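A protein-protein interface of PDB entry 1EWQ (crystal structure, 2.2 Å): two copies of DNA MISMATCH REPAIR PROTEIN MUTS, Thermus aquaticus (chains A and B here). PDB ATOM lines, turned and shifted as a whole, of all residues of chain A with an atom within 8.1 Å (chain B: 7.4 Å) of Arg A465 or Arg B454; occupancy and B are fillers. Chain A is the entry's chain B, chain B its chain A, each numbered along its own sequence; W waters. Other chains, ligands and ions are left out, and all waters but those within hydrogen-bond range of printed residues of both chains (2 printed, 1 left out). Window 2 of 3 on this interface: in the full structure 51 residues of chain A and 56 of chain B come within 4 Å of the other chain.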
ATOM      1  N   TYR A 449     -16.732 -37.832  -2.112  1.00  0.00           N
ATOM      2  CA  TYR A 449     -16.518 -36.399  -2.028  1.00  0.00           C
ATOM      3  C   TYR A 449     -17.676 -35.675  -1.372  1.00  0.00           C
ATOM      4  O   TYR A 449     -18.720 -36.261  -1.077  1.00  0.00           O
ATOM      5  CB  TYR A 449     -16.335 -35.857  -3.439  1.00  0.00           C
ATOM      6  CG  TYR A 449     -17.468 -36.257  -4.366  1.00  0.00           C
ATOM      7  CD1 TYR A 449     -18.718 -35.643  -4.279  1.00  0.00           C
ATOM      8  CD2 TYR A 449     -17.295 -37.263  -5.321  1.00  0.00           C
ATOM      9  CE1 TYR A 449     -19.765 -36.014  -5.120  1.00  0.00           C
ATOM     10  CE2 TYR A 449     -18.338 -37.642  -6.166  1.00  0.00           C
ATOM     11  CZ  TYR A 449     -19.568 -37.012  -6.060  1.00  0.00           C
ATOM     12  OH  TYR A 449     -20.602 -37.361  -6.896  1.00  0.00           O
ATOM     13  N   LEU A 450     -17.470 -34.386  -1.145  1.00  0.00           N
ATOM     14  CA  LEU A 450     -18.486 -33.520  -0.571  1.00  0.00           C
ATOM     15  C   LEU A 450     -18.829 -32.592  -1.720  1.00  0.00           C
ATOM     16  O   LEU A 450     -17.957 -32.222  -2.505  1.00  0.00           O
ATOM     17  CB  LEU A 450     -17.920 -32.734   0.612  1.00  0.00           C
ATOM     18  CG  LEU A 450     -17.619 -33.577   1.852  1.00  0.00           C
ATOM     19  CD1 LEU A 450     -16.783 -32.776   2.827  1.00  0.00           C
ATOM     20  CD2 LEU A 450     -18.927 -34.030   2.498  1.00  0.00           C
ATOM     21  N   VAL A 460     -17.869 -22.620   2.277  1.00  0.00           N
ATOM     22  CA  VAL A 460     -17.068 -23.835   2.353  1.00  0.00           C
ATOM     23  C   VAL A 460     -15.858 -23.587   3.240  1.00  0.00           C
ATOM     24  O   VAL A 460     -15.115 -22.631   3.029  1.00  0.00           O
ATOM     25  CB  VAL A 460     -16.570 -24.265   0.950  1.00  0.00           C
ATOM     26  CG1 VAL A 460     -15.466 -25.311   1.082  1.00  0.00           C
ATOM     27  CG2 VAL A 460     -17.728 -24.818   0.131  1.00  0.00           C
ATOM     28  N   PRO A 461     -15.648 -24.442   4.251  1.00  0.00           N
ATOM     29  CA  PRO A 461     -14.499 -24.264   5.142  1.00  0.00           C
ATOM     30  C   PRO A 461     -13.185 -24.475   4.400  1.00  0.00           C
ATOM     31  O   PRO A 461     -13.156 -25.062   3.315  1.00  0.00           O
ATOM     32  CB  PRO A 461     -14.738 -25.307   6.233  1.00  0.00           C
ATOM     33  CG  PRO A 461     -15.485 -26.381   5.520  1.00  0.00           C
ATOM     34  CD  PRO A 461     -16.455 -25.607   4.655  1.00  0.00           C
ATOM     35  N   LYS A 462     -12.098 -23.998   4.995  1.00  0.00           N
ATOM     36  CA  LYS A 462     -10.785 -24.112   4.383  1.00  0.00           C
ATOM     37  C   LYS A 462     -10.179 -25.510   4.482  1.00  0.00           C
ATOM     38  O   LYS A 462      -9.291 -25.861   3.707  1.00  0.00           O
ATOM     39  CB  LYS A 462      -9.861 -23.054   4.987  1.00  0.00           C
ATOM     40  CG  LYS A 462     -10.401 -21.646   4.779  1.00  0.00           C
ATOM     41  CD  LYS A 462      -9.276 -20.664   4.496  1.00  0.00           C
ATOM     42  CE  LYS A 462      -9.814 -19.323   4.008  1.00  0.00           C
ATOM     43  NZ  LYS A 462     -10.488 -19.470   2.688  1.00  0.00           N
ATOM     44  N   GLU A 463     -10.664 -26.307   5.429  1.00  0.00           N
ATOM     45  CA  GLU A 463     -10.179 -27.675   5.588  1.00  0.00           C
ATOM     46  C   GLU A 463     -10.476 -28.459   4.305  1.00  0.00           C
ATOM     47  O   GLU A 463      -9.772 -29.406   3.968  1.00  0.00           O
ATOM     48  CB  GLU A 463     -10.868 -28.367   6.770  1.00  0.00           C
ATOM     49  CG  GLU A 463     -10.453 -27.878   8.153  1.00  0.00           C
ATOM     50  CD  GLU A 463     -10.989 -26.499   8.499  1.00  0.00           C
ATOM     51  OE1 GLU A 463     -12.209 -26.268   8.355  1.00  0.00           O
ATOM     52  OE2 GLU A 463     -10.189 -25.646   8.933  1.00  0.00           O
ATOM     53  N   TYR A 464     -11.532 -28.055   3.600  1.00  0.00           N
ATOM     54  CA  TYR A 464     -11.936 -28.700   2.350  1.00  0.00           C
ATOM     55  C   TYR A 464     -10.891 -28.534   1.255  1.00  0.00           C
ATOM     56  O   TYR A 464     -10.319 -27.456   1.081  1.00  0.00           O
ATOM     57  CB  TYR A 464     -13.252 -28.108   1.839  1.00  0.00           C
ATOM     58  CG  TYR A 464     -14.504 -28.622   2.509  1.00  0.00           C
ATOM     59  CD1 TYR A 464     -14.484 -29.077   3.826  1.00  0.00           C
ATOM     60  CD2 TYR A 464     -15.729 -28.599   1.837  1.00  0.00           C
ATOM     61  CE1 TYR A 464     -15.652 -29.492   4.462  1.00  0.00           C
ATOM     62  CE2 TYR A 464     -16.906 -29.009   2.462  1.00  0.00           C
ATOM     63  CZ  TYR A 464     -16.860 -29.453   3.774  1.00  0.00           C
ATOM     64  OH  TYR A 464     -18.020 -29.845   4.406  1.00  0.00           O
ATOM     65  N   ARG A 465     -10.647 -29.614   0.524  1.00  0.00           N
ATOM     66  CA  ARG A 465      -9.708 -29.600  -0.589  1.00  0.00           C
ATOM     67  C   ARG A 465     -10.537 -29.864  -1.835  1.00  0.00           C
ATOM     68  O   ARG A 465     -11.053 -30.971  -2.019  1.00  0.00           O
ATOM     69  CB  ARG A 465      -8.662 -30.706  -0.444  1.00  0.00           C
ATOM     70  CG  ARG A 465      -7.914 -31.024  -1.740  1.00  0.00           C
ATOM     71  CD  ARG A 465      -7.203 -32.365  -1.632  1.00  0.00           C
ATOM     72  NE  ARG A 465      -6.723 -32.877  -2.918  1.00  0.00           N
ATOM     73  CZ  ARG A 465      -5.710 -32.361  -3.611  1.00  0.00           C
ATOM     74  NH1 ARG A 465      -5.050 -31.302  -3.150  1.00  0.00           N
ATOM     75  NH2 ARG A 465      -5.346 -32.913  -4.763  1.00  0.00           N
ATOM     76  N   PRO A 466     -10.695 -28.850  -2.701  1.00  0.00           N
ATOM     77  CA  PRO A 466     -11.482 -29.047  -3.921  1.00  0.00           C
ATOM     78  C   PRO A 466     -10.768 -30.072  -4.788  1.00  0.00           C
ATOM     79  O   PRO A 466      -9.540 -30.128  -4.796  1.00  0.00           O
ATOM     80  CB  PRO A 466     -11.483 -27.658  -4.548  1.00  0.00           C
ATOM     81  CG  PRO A 466     -10.119 -27.151  -4.188  1.00  0.00           C
ATOM     82  CD  PRO A 466     -10.017 -27.542  -2.720  1.00  0.00           C
ATOM     83  N   VAL A 467     -11.533 -30.881  -5.514  1.00  0.00           N
ATOM     84  CA  VAL A 467     -10.953 -31.905  -6.374  1.00  0.00           C
ATOM     85  C   VAL A 467     -11.555 -31.890  -7.774  1.00  0.00           C
ATOM     86  O   VAL A 467     -10.929 -32.355  -8.733  1.00  0.00           O
ATOM     87  CB  VAL A 467     -11.158 -33.307  -5.765  1.00  0.00           C
ATOM     88  CG1 VAL A 467     -10.400 -34.342  -6.585  1.00  0.00           C
ATOM     89  CG2 VAL A 467     -10.687 -33.316  -4.319  1.00  0.00           C
ATOM     90  N   GLN A 468     -12.770 -31.363  -7.893  1.00  0.00           N
ATOM     91  CA  GLN A 468     -13.437 -31.295  -9.186  1.00  0.00           C
ATOM     92  C   GLN A 468     -14.487 -30.193  -9.206  1.00  0.00           C
ATOM     93  O   GLN A 468     -15.279 -30.052  -8.270  1.00  0.00           O
ATOM     94  CB  GLN A 468     -14.086 -32.640  -9.521  1.00  0.00           C
ATOM     95  CG  GLN A 468     -14.871 -32.632 -10.820  1.00  0.00           C
ATOM     96  CD  GLN A 468     -15.465 -33.987 -11.167  1.00  0.00           C
ATOM     97  OE1 GLN A 468     -16.101 -34.635 -10.331  1.00  0.00           O
ATOM     98  NE2 GLN A 468     -15.267 -34.416 -12.409  1.00  0.00           N
ATOM     99  N   GLN A 474     -19.181 -27.810  -6.959  1.00  0.00           N
ATOM    100  CA  GLN A 474     -17.806 -28.244  -6.817  1.00  0.00           C
ATOM    101  C   GLN A 474     -17.728 -29.343  -5.766  1.00  0.00           C
ATOM    102  O   GLN A 474     -18.500 -29.355  -4.804  1.00  0.00           O
ATOM    103  CB  GLN A 474     -16.943 -27.047  -6.415  1.00  0.00           C
ATOM    104  CG  GLN A 474     -15.504 -27.119  -6.863  1.00  0.00           C
ATOM    105  CD  GLN A 474     -14.778 -25.806  -6.653  1.00  0.00           C
ATOM    106  OE1 GLN A 474     -13.609 -25.669  -7.005  1.00  0.00           O
ATOM    107  NE2 GLN A 474     -15.471 -24.830  -6.073  1.00  0.00           N
ATOM    108  N   ARG A 475     -16.789 -30.261  -5.954  1.00  0.00           N
ATOM    109  CA  ARG A 475     -16.617 -31.375  -5.036  1.00  0.00           C
ATOM    110  C   ARG A 475     -15.298 -31.275  -4.275  1.00  0.00           C
ATOM    111  O   ARG A 475     -14.235 -31.074  -4.866  1.00  0.00           O
ATOM    112  CB  ARG A 475     -16.709 -32.683  -5.825  1.00  0.00           C
ATOM    113  CG  ARG A 475     -18.062 -32.843  -6.493  1.00  0.00           C
ATOM    114  CD  ARG A 475     -18.095 -33.940  -7.536  1.00  0.00           C
ATOM    115  NE  ARG A 475     -19.415 -33.997  -8.155  1.00  0.00           N
ATOM    116  CZ  ARG A 475     -19.727 -34.733  -9.214  1.00  0.00           C
ATOM    117  NH1 ARG A 475     -18.810 -35.496  -9.794  1.00  0.00           N
ATOM    118  NH2 ARG A 475     -20.961 -34.696  -9.703  1.00  0.00           N
ATOM    119  N   TYR A 476     -15.383 -31.401  -2.955  1.00  0.00           N
ATOM    120  CA  TYR A 476     -14.210 -31.307  -2.097  1.00  0.00           C
ATOM    121  C   TYR A 476     -13.915 -32.618  -1.383  1.00  0.00           C
ATOM    122  O   TYR A 476     -14.671 -33.584  -1.490  1.00  0.00           O
ATOM    123  CB  TYR A 476     -14.403 -30.207  -1.053  1.00  0.00           C
ATOM    124  CG  TYR A 476     -14.866 -28.888  -1.623  1.00  0.00           C
ATOM    125  CD1 TYR A 476     -16.196 -28.698  -2.001  1.00  0.00           C
ATOM    126  CD2 TYR A 476     -13.980 -27.820  -1.772  1.00  0.00           C
ATOM    127  CE1 TYR A 476     -16.634 -27.476  -2.509  1.00  0.00           C
ATOM    128  CE2 TYR A 476     -14.407 -26.596  -2.280  1.00  0.00           C
ATOM    129  CZ  TYR A 476     -15.735 -26.432  -2.644  1.00  0.00           C
ATOM    130  OH  TYR A 476     -16.172 -25.226  -3.129  1.00  0.00           O
ATOM    131  N   THR A 477     -12.813 -32.628  -0.637  1.00  0.00           N
ATOM    132  CA  THR A 477     -12.368 -33.802   0.109  1.00  0.00           C
ATOM    133  C   THR A 477     -12.001 -33.426   1.538  1.00  0.00           C
ATOM    134  O   THR A 477     -11.668 -32.271   1.817  1.00  0.00           O
ATOM    135  CB  THR A 477     -11.133 -34.439  -0.580  1.00  0.00           C
ATOM    136  OG1 THR A 477     -11.520 -34.968  -1.854  1.00  0.00           O
ATOM    137  CG2 THR A 477     -10.548 -35.552   0.265  1.00  0.00           C
ATOM    138  N   LEU A 478     -12.070 -34.407   2.435  1.00  0.00           N
ATOM    139  CA  LEU A 478     -11.733 -34.212   3.843  1.00  0.00           C
ATOM    140  C   LEU A 478     -10.854 -35.383   4.283  1.00  0.00           C
ATOM    141  O   LEU A 478     -11.142 -36.536   3.961  1.00  0.00           O
ATOM    142  CB  LEU A 478     -13.013 -34.150   4.686  1.00  0.00           C
ATOM    143  CG  LEU A 478     -13.179 -32.969   5.652  1.00  0.00           C
ATOM    144  CD1 LEU A 478     -12.776 -31.672   4.965  1.00  0.00           C
ATOM    145  CD2 LEU A 478     -14.630 -32.896   6.129  1.00  0.00           C
ATOM    146  N   PRO A 479      -9.772 -35.100   5.027  1.00  0.00           N
ATOM    147  CA  PRO A 479      -8.813 -36.095   5.528  1.00  0.00           C
ATOM    148  C   PRO A 479      -9.336 -37.456   6.018  1.00  0.00           C
ATOM    149  O   PRO A 479      -8.811 -38.501   5.624  1.00  0.00           O
ATOM    150  CB  PRO A 479      -8.079 -35.329   6.624  1.00  0.00           C
ATOM    151  CG  PRO A 479      -8.024 -33.935   6.047  1.00  0.00           C
ATOM    152  CD  PRO A 479      -9.430 -33.750   5.516  1.00  0.00           C
ATOM    153  N   VAL B 452      -3.028 -24.429 -16.265  1.00  0.00           N
ATOM    154  CA  VAL B 452      -1.699 -24.739 -15.739  1.00  0.00           C
ATOM    155  C   VAL B 452      -1.763 -26.109 -15.072  1.00  0.00           C
ATOM    156  O   VAL B 452      -2.755 -26.446 -14.424  1.00  0.00           O
ATOM    157  CB  VAL B 452      -1.247 -23.697 -14.680  1.00  0.00           C
ATOM    158  CG1 VAL B 452       0.064 -24.135 -14.041  1.00  0.00           C
ATOM    159  CG2 VAL B 452      -1.071 -22.322 -15.327  1.00  0.00           C
ATOM    160  N   THR B 453      -0.709 -26.897 -15.237  1.00  0.00           N
ATOM    161  CA  THR B 453      -0.630 -28.229 -14.636  1.00  0.00           C
ATOM    162  C   THR B 453      -0.106 -28.161 -13.196  1.00  0.00           C
ATOM    163  O   THR B 453       0.561 -27.197 -12.809  1.00  0.00           O
ATOM    164  CB  THR B 453       0.312 -29.140 -15.430  1.00  0.00           C
ATOM    165  OG1 THR B 453       1.631 -28.575 -15.422  1.00  0.00           O
ATOM    166  CG2 THR B 453      -0.174 -29.286 -16.863  1.00  0.00           C
ATOM    167  N   ARG B 454      -0.403 -29.209 -12.430  1.00  0.00           N
ATOM    168  CA  ARG B 454      -0.008 -29.330 -11.033  1.00  0.00           C
ATOM    169  C   ARG B 454       1.412 -28.883 -10.694  1.00  0.00           C
ATOM    170  O   ARG B 454       1.607 -28.136  -9.741  1.00  0.00           O
ATOM    171  CB  ARG B 454      -0.217 -30.775 -10.551  1.00  0.00           C
ATOM    172  CG  ARG B 454       0.052 -30.985  -9.057  1.00  0.00           C
ATOM    173  CD  ARG B 454      -0.286 -32.403  -8.626  1.00  0.00           C
ATOM    174  NE  ARG B 454      -1.727 -32.654  -8.638  1.00  0.00           N
ATOM    175  CZ  ARG B 454      -2.594 -32.094  -7.799  1.00  0.00           C
ATOM    176  NH1 ARG B 454      -2.177 -31.244  -6.871  1.00  0.00           N
ATOM    177  NH2 ARG B 454      -3.884 -32.383  -7.893  1.00  0.00           N
ATOM    178  N   PRO B 455       2.421 -29.321 -11.473  1.00  0.00           N
ATOM    179  CA  PRO B 455       3.805 -28.927 -11.196  1.00  0.00           C
ATOM    180  C   PRO B 455       4.059 -27.417 -11.160  1.00  0.00           C
ATOM    181  O   PRO B 455       5.107 -26.971 -10.680  1.00  0.00           O
ATOM    182  CB  PRO B 455       4.593 -29.623 -12.309  1.00  0.00           C
ATOM    183  CG  PRO B 455       3.784 -30.851 -12.567  1.00  0.00           C
ATOM    184  CD  PRO B 455       2.376 -30.294 -12.579  1.00  0.00           C
ATOM    185  N   TYR B 456       3.122 -26.623 -11.664  1.00  0.00           N
ATOM    186  CA  TYR B 456       3.321 -25.181 -11.637  1.00  0.00           C
ATOM    187  C   TYR B 456       2.295 -24.427 -10.800  1.00  0.00           C
ATOM    188  O   TYR B 456       2.240 -23.204 -10.868  1.00  0.00           O
ATOM    189  CB  TYR B 456       3.336 -24.604 -13.056  1.00  0.00           C
ATOM    190  CG  TYR B 456       4.431 -25.164 -13.936  1.00  0.00           C
ATOM    191  CD1 TYR B 456       4.238 -26.339 -14.662  1.00  0.00           C
ATOM    192  CD2 TYR B 456       5.673 -24.533 -14.024  1.00  0.00           C
ATOM    193  CE1 TYR B 456       5.255 -26.870 -15.451  1.00  0.00           C
ATOM    194  CE2 TYR B 456       6.700 -25.055 -14.811  1.00  0.00           C
ATOM    195  CZ  TYR B 456       6.487 -26.221 -15.517  1.00  0.00           C
ATOM    196  OH  TYR B 456       7.509 -26.760 -16.271  1.00  0.00           O
ATOM    197  N   TYR B 457       1.491 -25.138 -10.011  1.00  0.00           N
ATOM    198  CA  TYR B 457       0.486 -24.479  -9.176  1.00  0.00           C
ATOM    199  C   TYR B 457       1.022 -23.346  -8.283  1.00  0.00           C
ATOM    200  O   TYR B 457       0.373 -22.318  -8.152  1.00  0.00           O
ATOM    201  CB  TYR B 457      -0.246 -25.497  -8.285  1.00  0.00           C
ATOM    202  CG  TYR B 457      -1.259 -26.375  -9.004  1.00  0.00           C
ATOM    203  CD1 TYR B 457      -1.451 -26.279 -10.384  1.00  0.00           C
ATOM    204  CD2 TYR B 457      -2.009 -27.313  -8.298  1.00  0.00           C
ATOM    205  CE1 TYR B 457      -2.367 -27.105 -11.047  1.00  0.00           C
ATOM    206  CE2 TYR B 457      -2.931 -28.141  -8.942  1.00  0.00           C
ATOM    207  CZ  TYR B 457      -3.104 -28.037 -10.316  1.00  0.00           C
ATOM    208  OH  TYR B 457      -3.992 -28.870 -10.956  1.00  0.00           O
ATOM    209  N   GLU B 458       2.191 -23.527  -7.671  1.00  0.00           N
ATOM    210  CA  GLU B 458       2.756 -22.496  -6.788  1.00  0.00           C
ATOM    211  C   GLU B 458       3.426 -21.405  -7.623  1.00  0.00           C
ATOM    212  O   GLU B 458       4.019 -20.468  -7.093  1.00  0.00           O
ATOM    213  CB  GLU B 458       3.799 -23.108  -5.830  1.00  0.00           C
ATOM    214  CG  GLU B 458       3.449 -24.485  -5.268  1.00  0.00           C
ATOM    215  CD  GLU B 458       4.431 -24.954  -4.197  1.00  0.00           C
ATOM    216  OE1 GLU B 458       4.545 -26.170  -3.966  1.00  0.00           O
ATOM    217  OE2 GLU B 458       5.086 -24.104  -3.571  1.00  0.00           O
ATOM    218  N   ARG B 459       3.307 -21.540  -8.937  1.00  0.00           N
ATOM    219  CA  ARG B 459       3.911 -20.615  -9.883  1.00  0.00           C
ATOM    220  C   ARG B 459       2.862 -19.665 -10.501  1.00  0.00           C
ATOM    221  O   ARG B 459       3.198 -18.720 -11.219  1.00  0.00           O
ATOM    222  CB  ARG B 459       4.595 -21.457 -10.962  1.00  0.00           C
ATOM    223  CG  ARG B 459       5.982 -21.033 -11.347  1.00  0.00           C
ATOM    224  CD  ARG B 459       6.956 -20.905 -10.179  1.00  0.00           C
ATOM    225  NE  ARG B 459       7.981 -19.944 -10.573  1.00  0.00           N
ATOM    226  CZ  ARG B 459       8.849 -19.360  -9.757  1.00  0.00           C
ATOM    227  NH1 ARG B 459       8.852 -19.632  -8.461  1.00  0.00           N
ATOM    228  NH2 ARG B 459       9.695 -18.462 -10.244  1.00  0.00           N
ATOM    229  N   THR B 469     -11.325 -26.738 -11.316  1.00  0.00           N
ATOM    230  CA  THR B 469     -10.319 -27.610 -10.740  1.00  0.00           C
ATOM    231  C   THR B 469     -10.473 -28.990 -11.367  1.00  0.00           C
ATOM    232  O   THR B 469     -11.582 -29.520 -11.474  1.00  0.00           O
ATOM    233  CB  THR B 469     -10.483 -27.757  -9.202  1.00  0.00           C
ATOM    234  OG1 THR B 469     -10.308 -26.481  -8.565  1.00  0.00           O
ATOM    235  CG2 THR B 469      -9.449 -28.743  -8.652  1.00  0.00           C
ATOM    236  N   LEU B 470      -9.358 -29.564 -11.795  1.00  0.00           N
ATOM    237  CA  LEU B 470      -9.390 -30.889 -12.390  1.00  0.00           C
ATOM    238  C   LEU B 470      -8.459 -31.803 -11.615  1.00  0.00           C
ATOM    239  O   LEU B 470      -7.825 -31.383 -10.648  1.00  0.00           O
ATOM    240  CB  LEU B 470      -8.990 -30.832 -13.872  1.00  0.00           C
ATOM    241  CG  LEU B 470      -9.950 -30.010 -14.737  1.00  0.00           C
ATOM    242  CD1 LEU B 470      -9.320 -28.662 -15.069  1.00  0.00           C
ATOM    243  CD2 LEU B 470     -10.276 -30.768 -16.009  1.00  0.00           C
ATOM    244  N   LYS B 471      -8.386 -33.055 -12.043  1.00  0.00           N
ATOM    245  CA  LYS B 471      -7.547 -34.034 -11.382  1.00  0.00           C
ATOM    246  C   LYS B 471      -6.127 -33.520 -11.159  1.00  0.00           C
ATOM    247  O   LYS B 471      -5.626 -33.554 -10.034  1.00  0.00           O
ATOM    248  CB  LYS B 471      -7.518 -35.334 -12.197  1.00  0.00           C
ATOM    249  CG  LYS B 471      -7.147 -36.577 -11.399  1.00  0.00           C
ATOM    250  CD  LYS B 471      -7.978 -36.688 -10.120  1.00  0.00           C
ATOM    251  CE  LYS B 471      -7.819 -38.061  -9.479  1.00  0.00           C
ATOM    252  NZ  LYS B 471      -6.381 -38.457  -9.352  1.00  0.00           N
ATOM    253  N   ASP B 472      -5.480 -33.042 -12.219  1.00  0.00           N
ATOM    254  CA  ASP B 472      -4.109 -32.552 -12.097  1.00  0.00           C
ATOM    255  C   ASP B 472      -3.845 -31.292 -12.910  1.00  0.00           C
ATOM    256  O   ASP B 472      -2.720 -31.028 -13.338  1.00  0.00           O
ATOM    257  CB  ASP B 472      -3.130 -33.650 -12.500  1.00  0.00           C
ATOM    258  CG  ASP B 472      -3.171 -34.835 -11.552  1.00  0.00           C
ATOM    259  OD1 ASP B 472      -2.749 -34.676 -10.380  1.00  0.00           O
ATOM    260  OD2 ASP B 472      -3.632 -35.916 -11.973  1.00  0.00           O
ATOM    261  N   ARG B 473      -4.907 -30.525 -13.114  1.00  0.00           N
ATOM    262  CA  ARG B 473      -4.828 -29.273 -13.842  1.00  0.00           C
ATOM    263  C   ARG B 473      -5.799 -28.327 -13.188  1.00  0.00           C
ATOM    264  O   ARG B 473      -6.757 -28.753 -12.543  1.00  0.00           O
ATOM    265  CB  ARG B 473      -5.195 -29.464 -15.315  1.00  0.00           C
ATOM    266  CG  ARG B 473      -4.132 -30.195 -16.130  1.00  0.00           C
ATOM    267  CD  ARG B 473      -4.654 -30.520 -17.504  1.00  0.00           C
ATOM    268  NE  ARG B 473      -5.799 -31.424 -17.435  1.00  0.00           N
ATOM    269  CZ  ARG B 473      -6.634 -31.656 -18.444  1.00  0.00           C
ATOM    270  NH1 ARG B 473      -6.459 -31.046 -19.616  1.00  0.00           N
ATOM    271  NH2 ARG B 473      -7.644 -32.506 -18.284  1.00  0.00           N
ATOM    272  N   GLN B 474      -5.537 -27.039 -13.346  1.00  0.00           N
ATOM    273  CA  GLN B 474      -6.392 -26.010 -12.782  1.00  0.00           C
ATOM    274  C   GLN B 474      -6.543 -24.921 -13.825  1.00  0.00           C
ATOM    275  O   GLN B 474      -5.582 -24.567 -14.517  1.00  0.00           O
ATOM    276  CB  GLN B 474      -5.768 -25.436 -11.507  1.00  0.00           C
ATOM    277  CG  GLN B 474      -6.528 -24.265 -10.893  1.00  0.00           C
ATOM    278  CD  GLN B 474      -7.912 -24.638 -10.371  1.00  0.00           C
ATOM    279  OE1 GLN B 474      -8.078 -25.638  -9.666  1.00  0.00           O
ATOM    280  NE2 GLN B 474      -8.910 -23.821 -10.703  1.00  0.00           N
HETATM  281  O   HOH W   1      -3.669 -29.757  -5.045  1.00  0.00           O
HETATM  282  O   HOH W   2     -11.518 -23.924  -9.093  1.00  0.00           O
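Arg A465 touches just one residue of chain B: Arg B454. Of the printed residues of chain A, Arg B454 touches Arg A465. No residue of chain A comes within 4 Å of Pro B455. Of the printed residues of chain A, Leu B470 touches Val A467 (3.8 Å). Of the printed residues of chain B, Gln A474 touches Thr B469. Of the printed residues of chain B, Gln A468 touches Thr B469. Pro A479 touches none of the printed residues of chain B. Lys A462 touches none of the printed residues of chain B. The nearest residue of chain B that does not touch Arg A465 is Lys B471 (5.3 Å). The nearest printed residue of chain B that does not touch Val A467 is Lys B471 (4.2 Å).
Among the printed residues, no Asp or Glu carboxylate lies within 4 Å of a Lys or Arg side-chain nitrogen of the other chain.
NH2 of Arg B454 sits close to NH2 of Arg A465 (3.5 Å).
Water W1 bridges the guanidinium group (NH1) of Arg B454 (2.8 Å) and the guanidinium group (NH1) of Arg A465 (2.8 Å). Water W2 lies within hydrogen-bond range of the side-chain hydroxyl (OG1) of Thr B469 (2.9 Å), the side-chain amide nitrogen (NE2) of Gln B474 (3.1 Å) and the side-chain amide oxygen (OE1) of Gln A474 (3.4 Å).
1 position is printed for both chains. Of the 5 pairs that touch across the chains among the printed residues, none has its exchanged pair printed and touching as well.
Among the printed residues, pairs that only touch across the chains: Gln A468 with Thr B469, Gln A474 with Thr B469, Val A467 with Leu B470 and Val A467 with Thr B469.
OD1 of Asp B472 is in salt-bridge range of NE of Arg B454 (2.9 Å). OE1 of Gln B474 lies within hydrogen-bond range of OG1 of Thr B469, at 2.6 Å. The backbone carbonyl oxygen (O) of Arg A465 sits at hydrogen-bond distance from the backbone NH (N) of Thr A477, 2.8 Å away. O of Arg A475 lies within hydrogen-bond range of N of Val A467 (2.8 Å). O of Gln A468 sits at hydrogen-bond distance from N of Arg A475, 2.8 Å away. The side-chain amide nitrogen (NE2) of Gln A474 is in hydrogen-bond range of the side-chain hydroxyl (OH) of Tyr A476.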
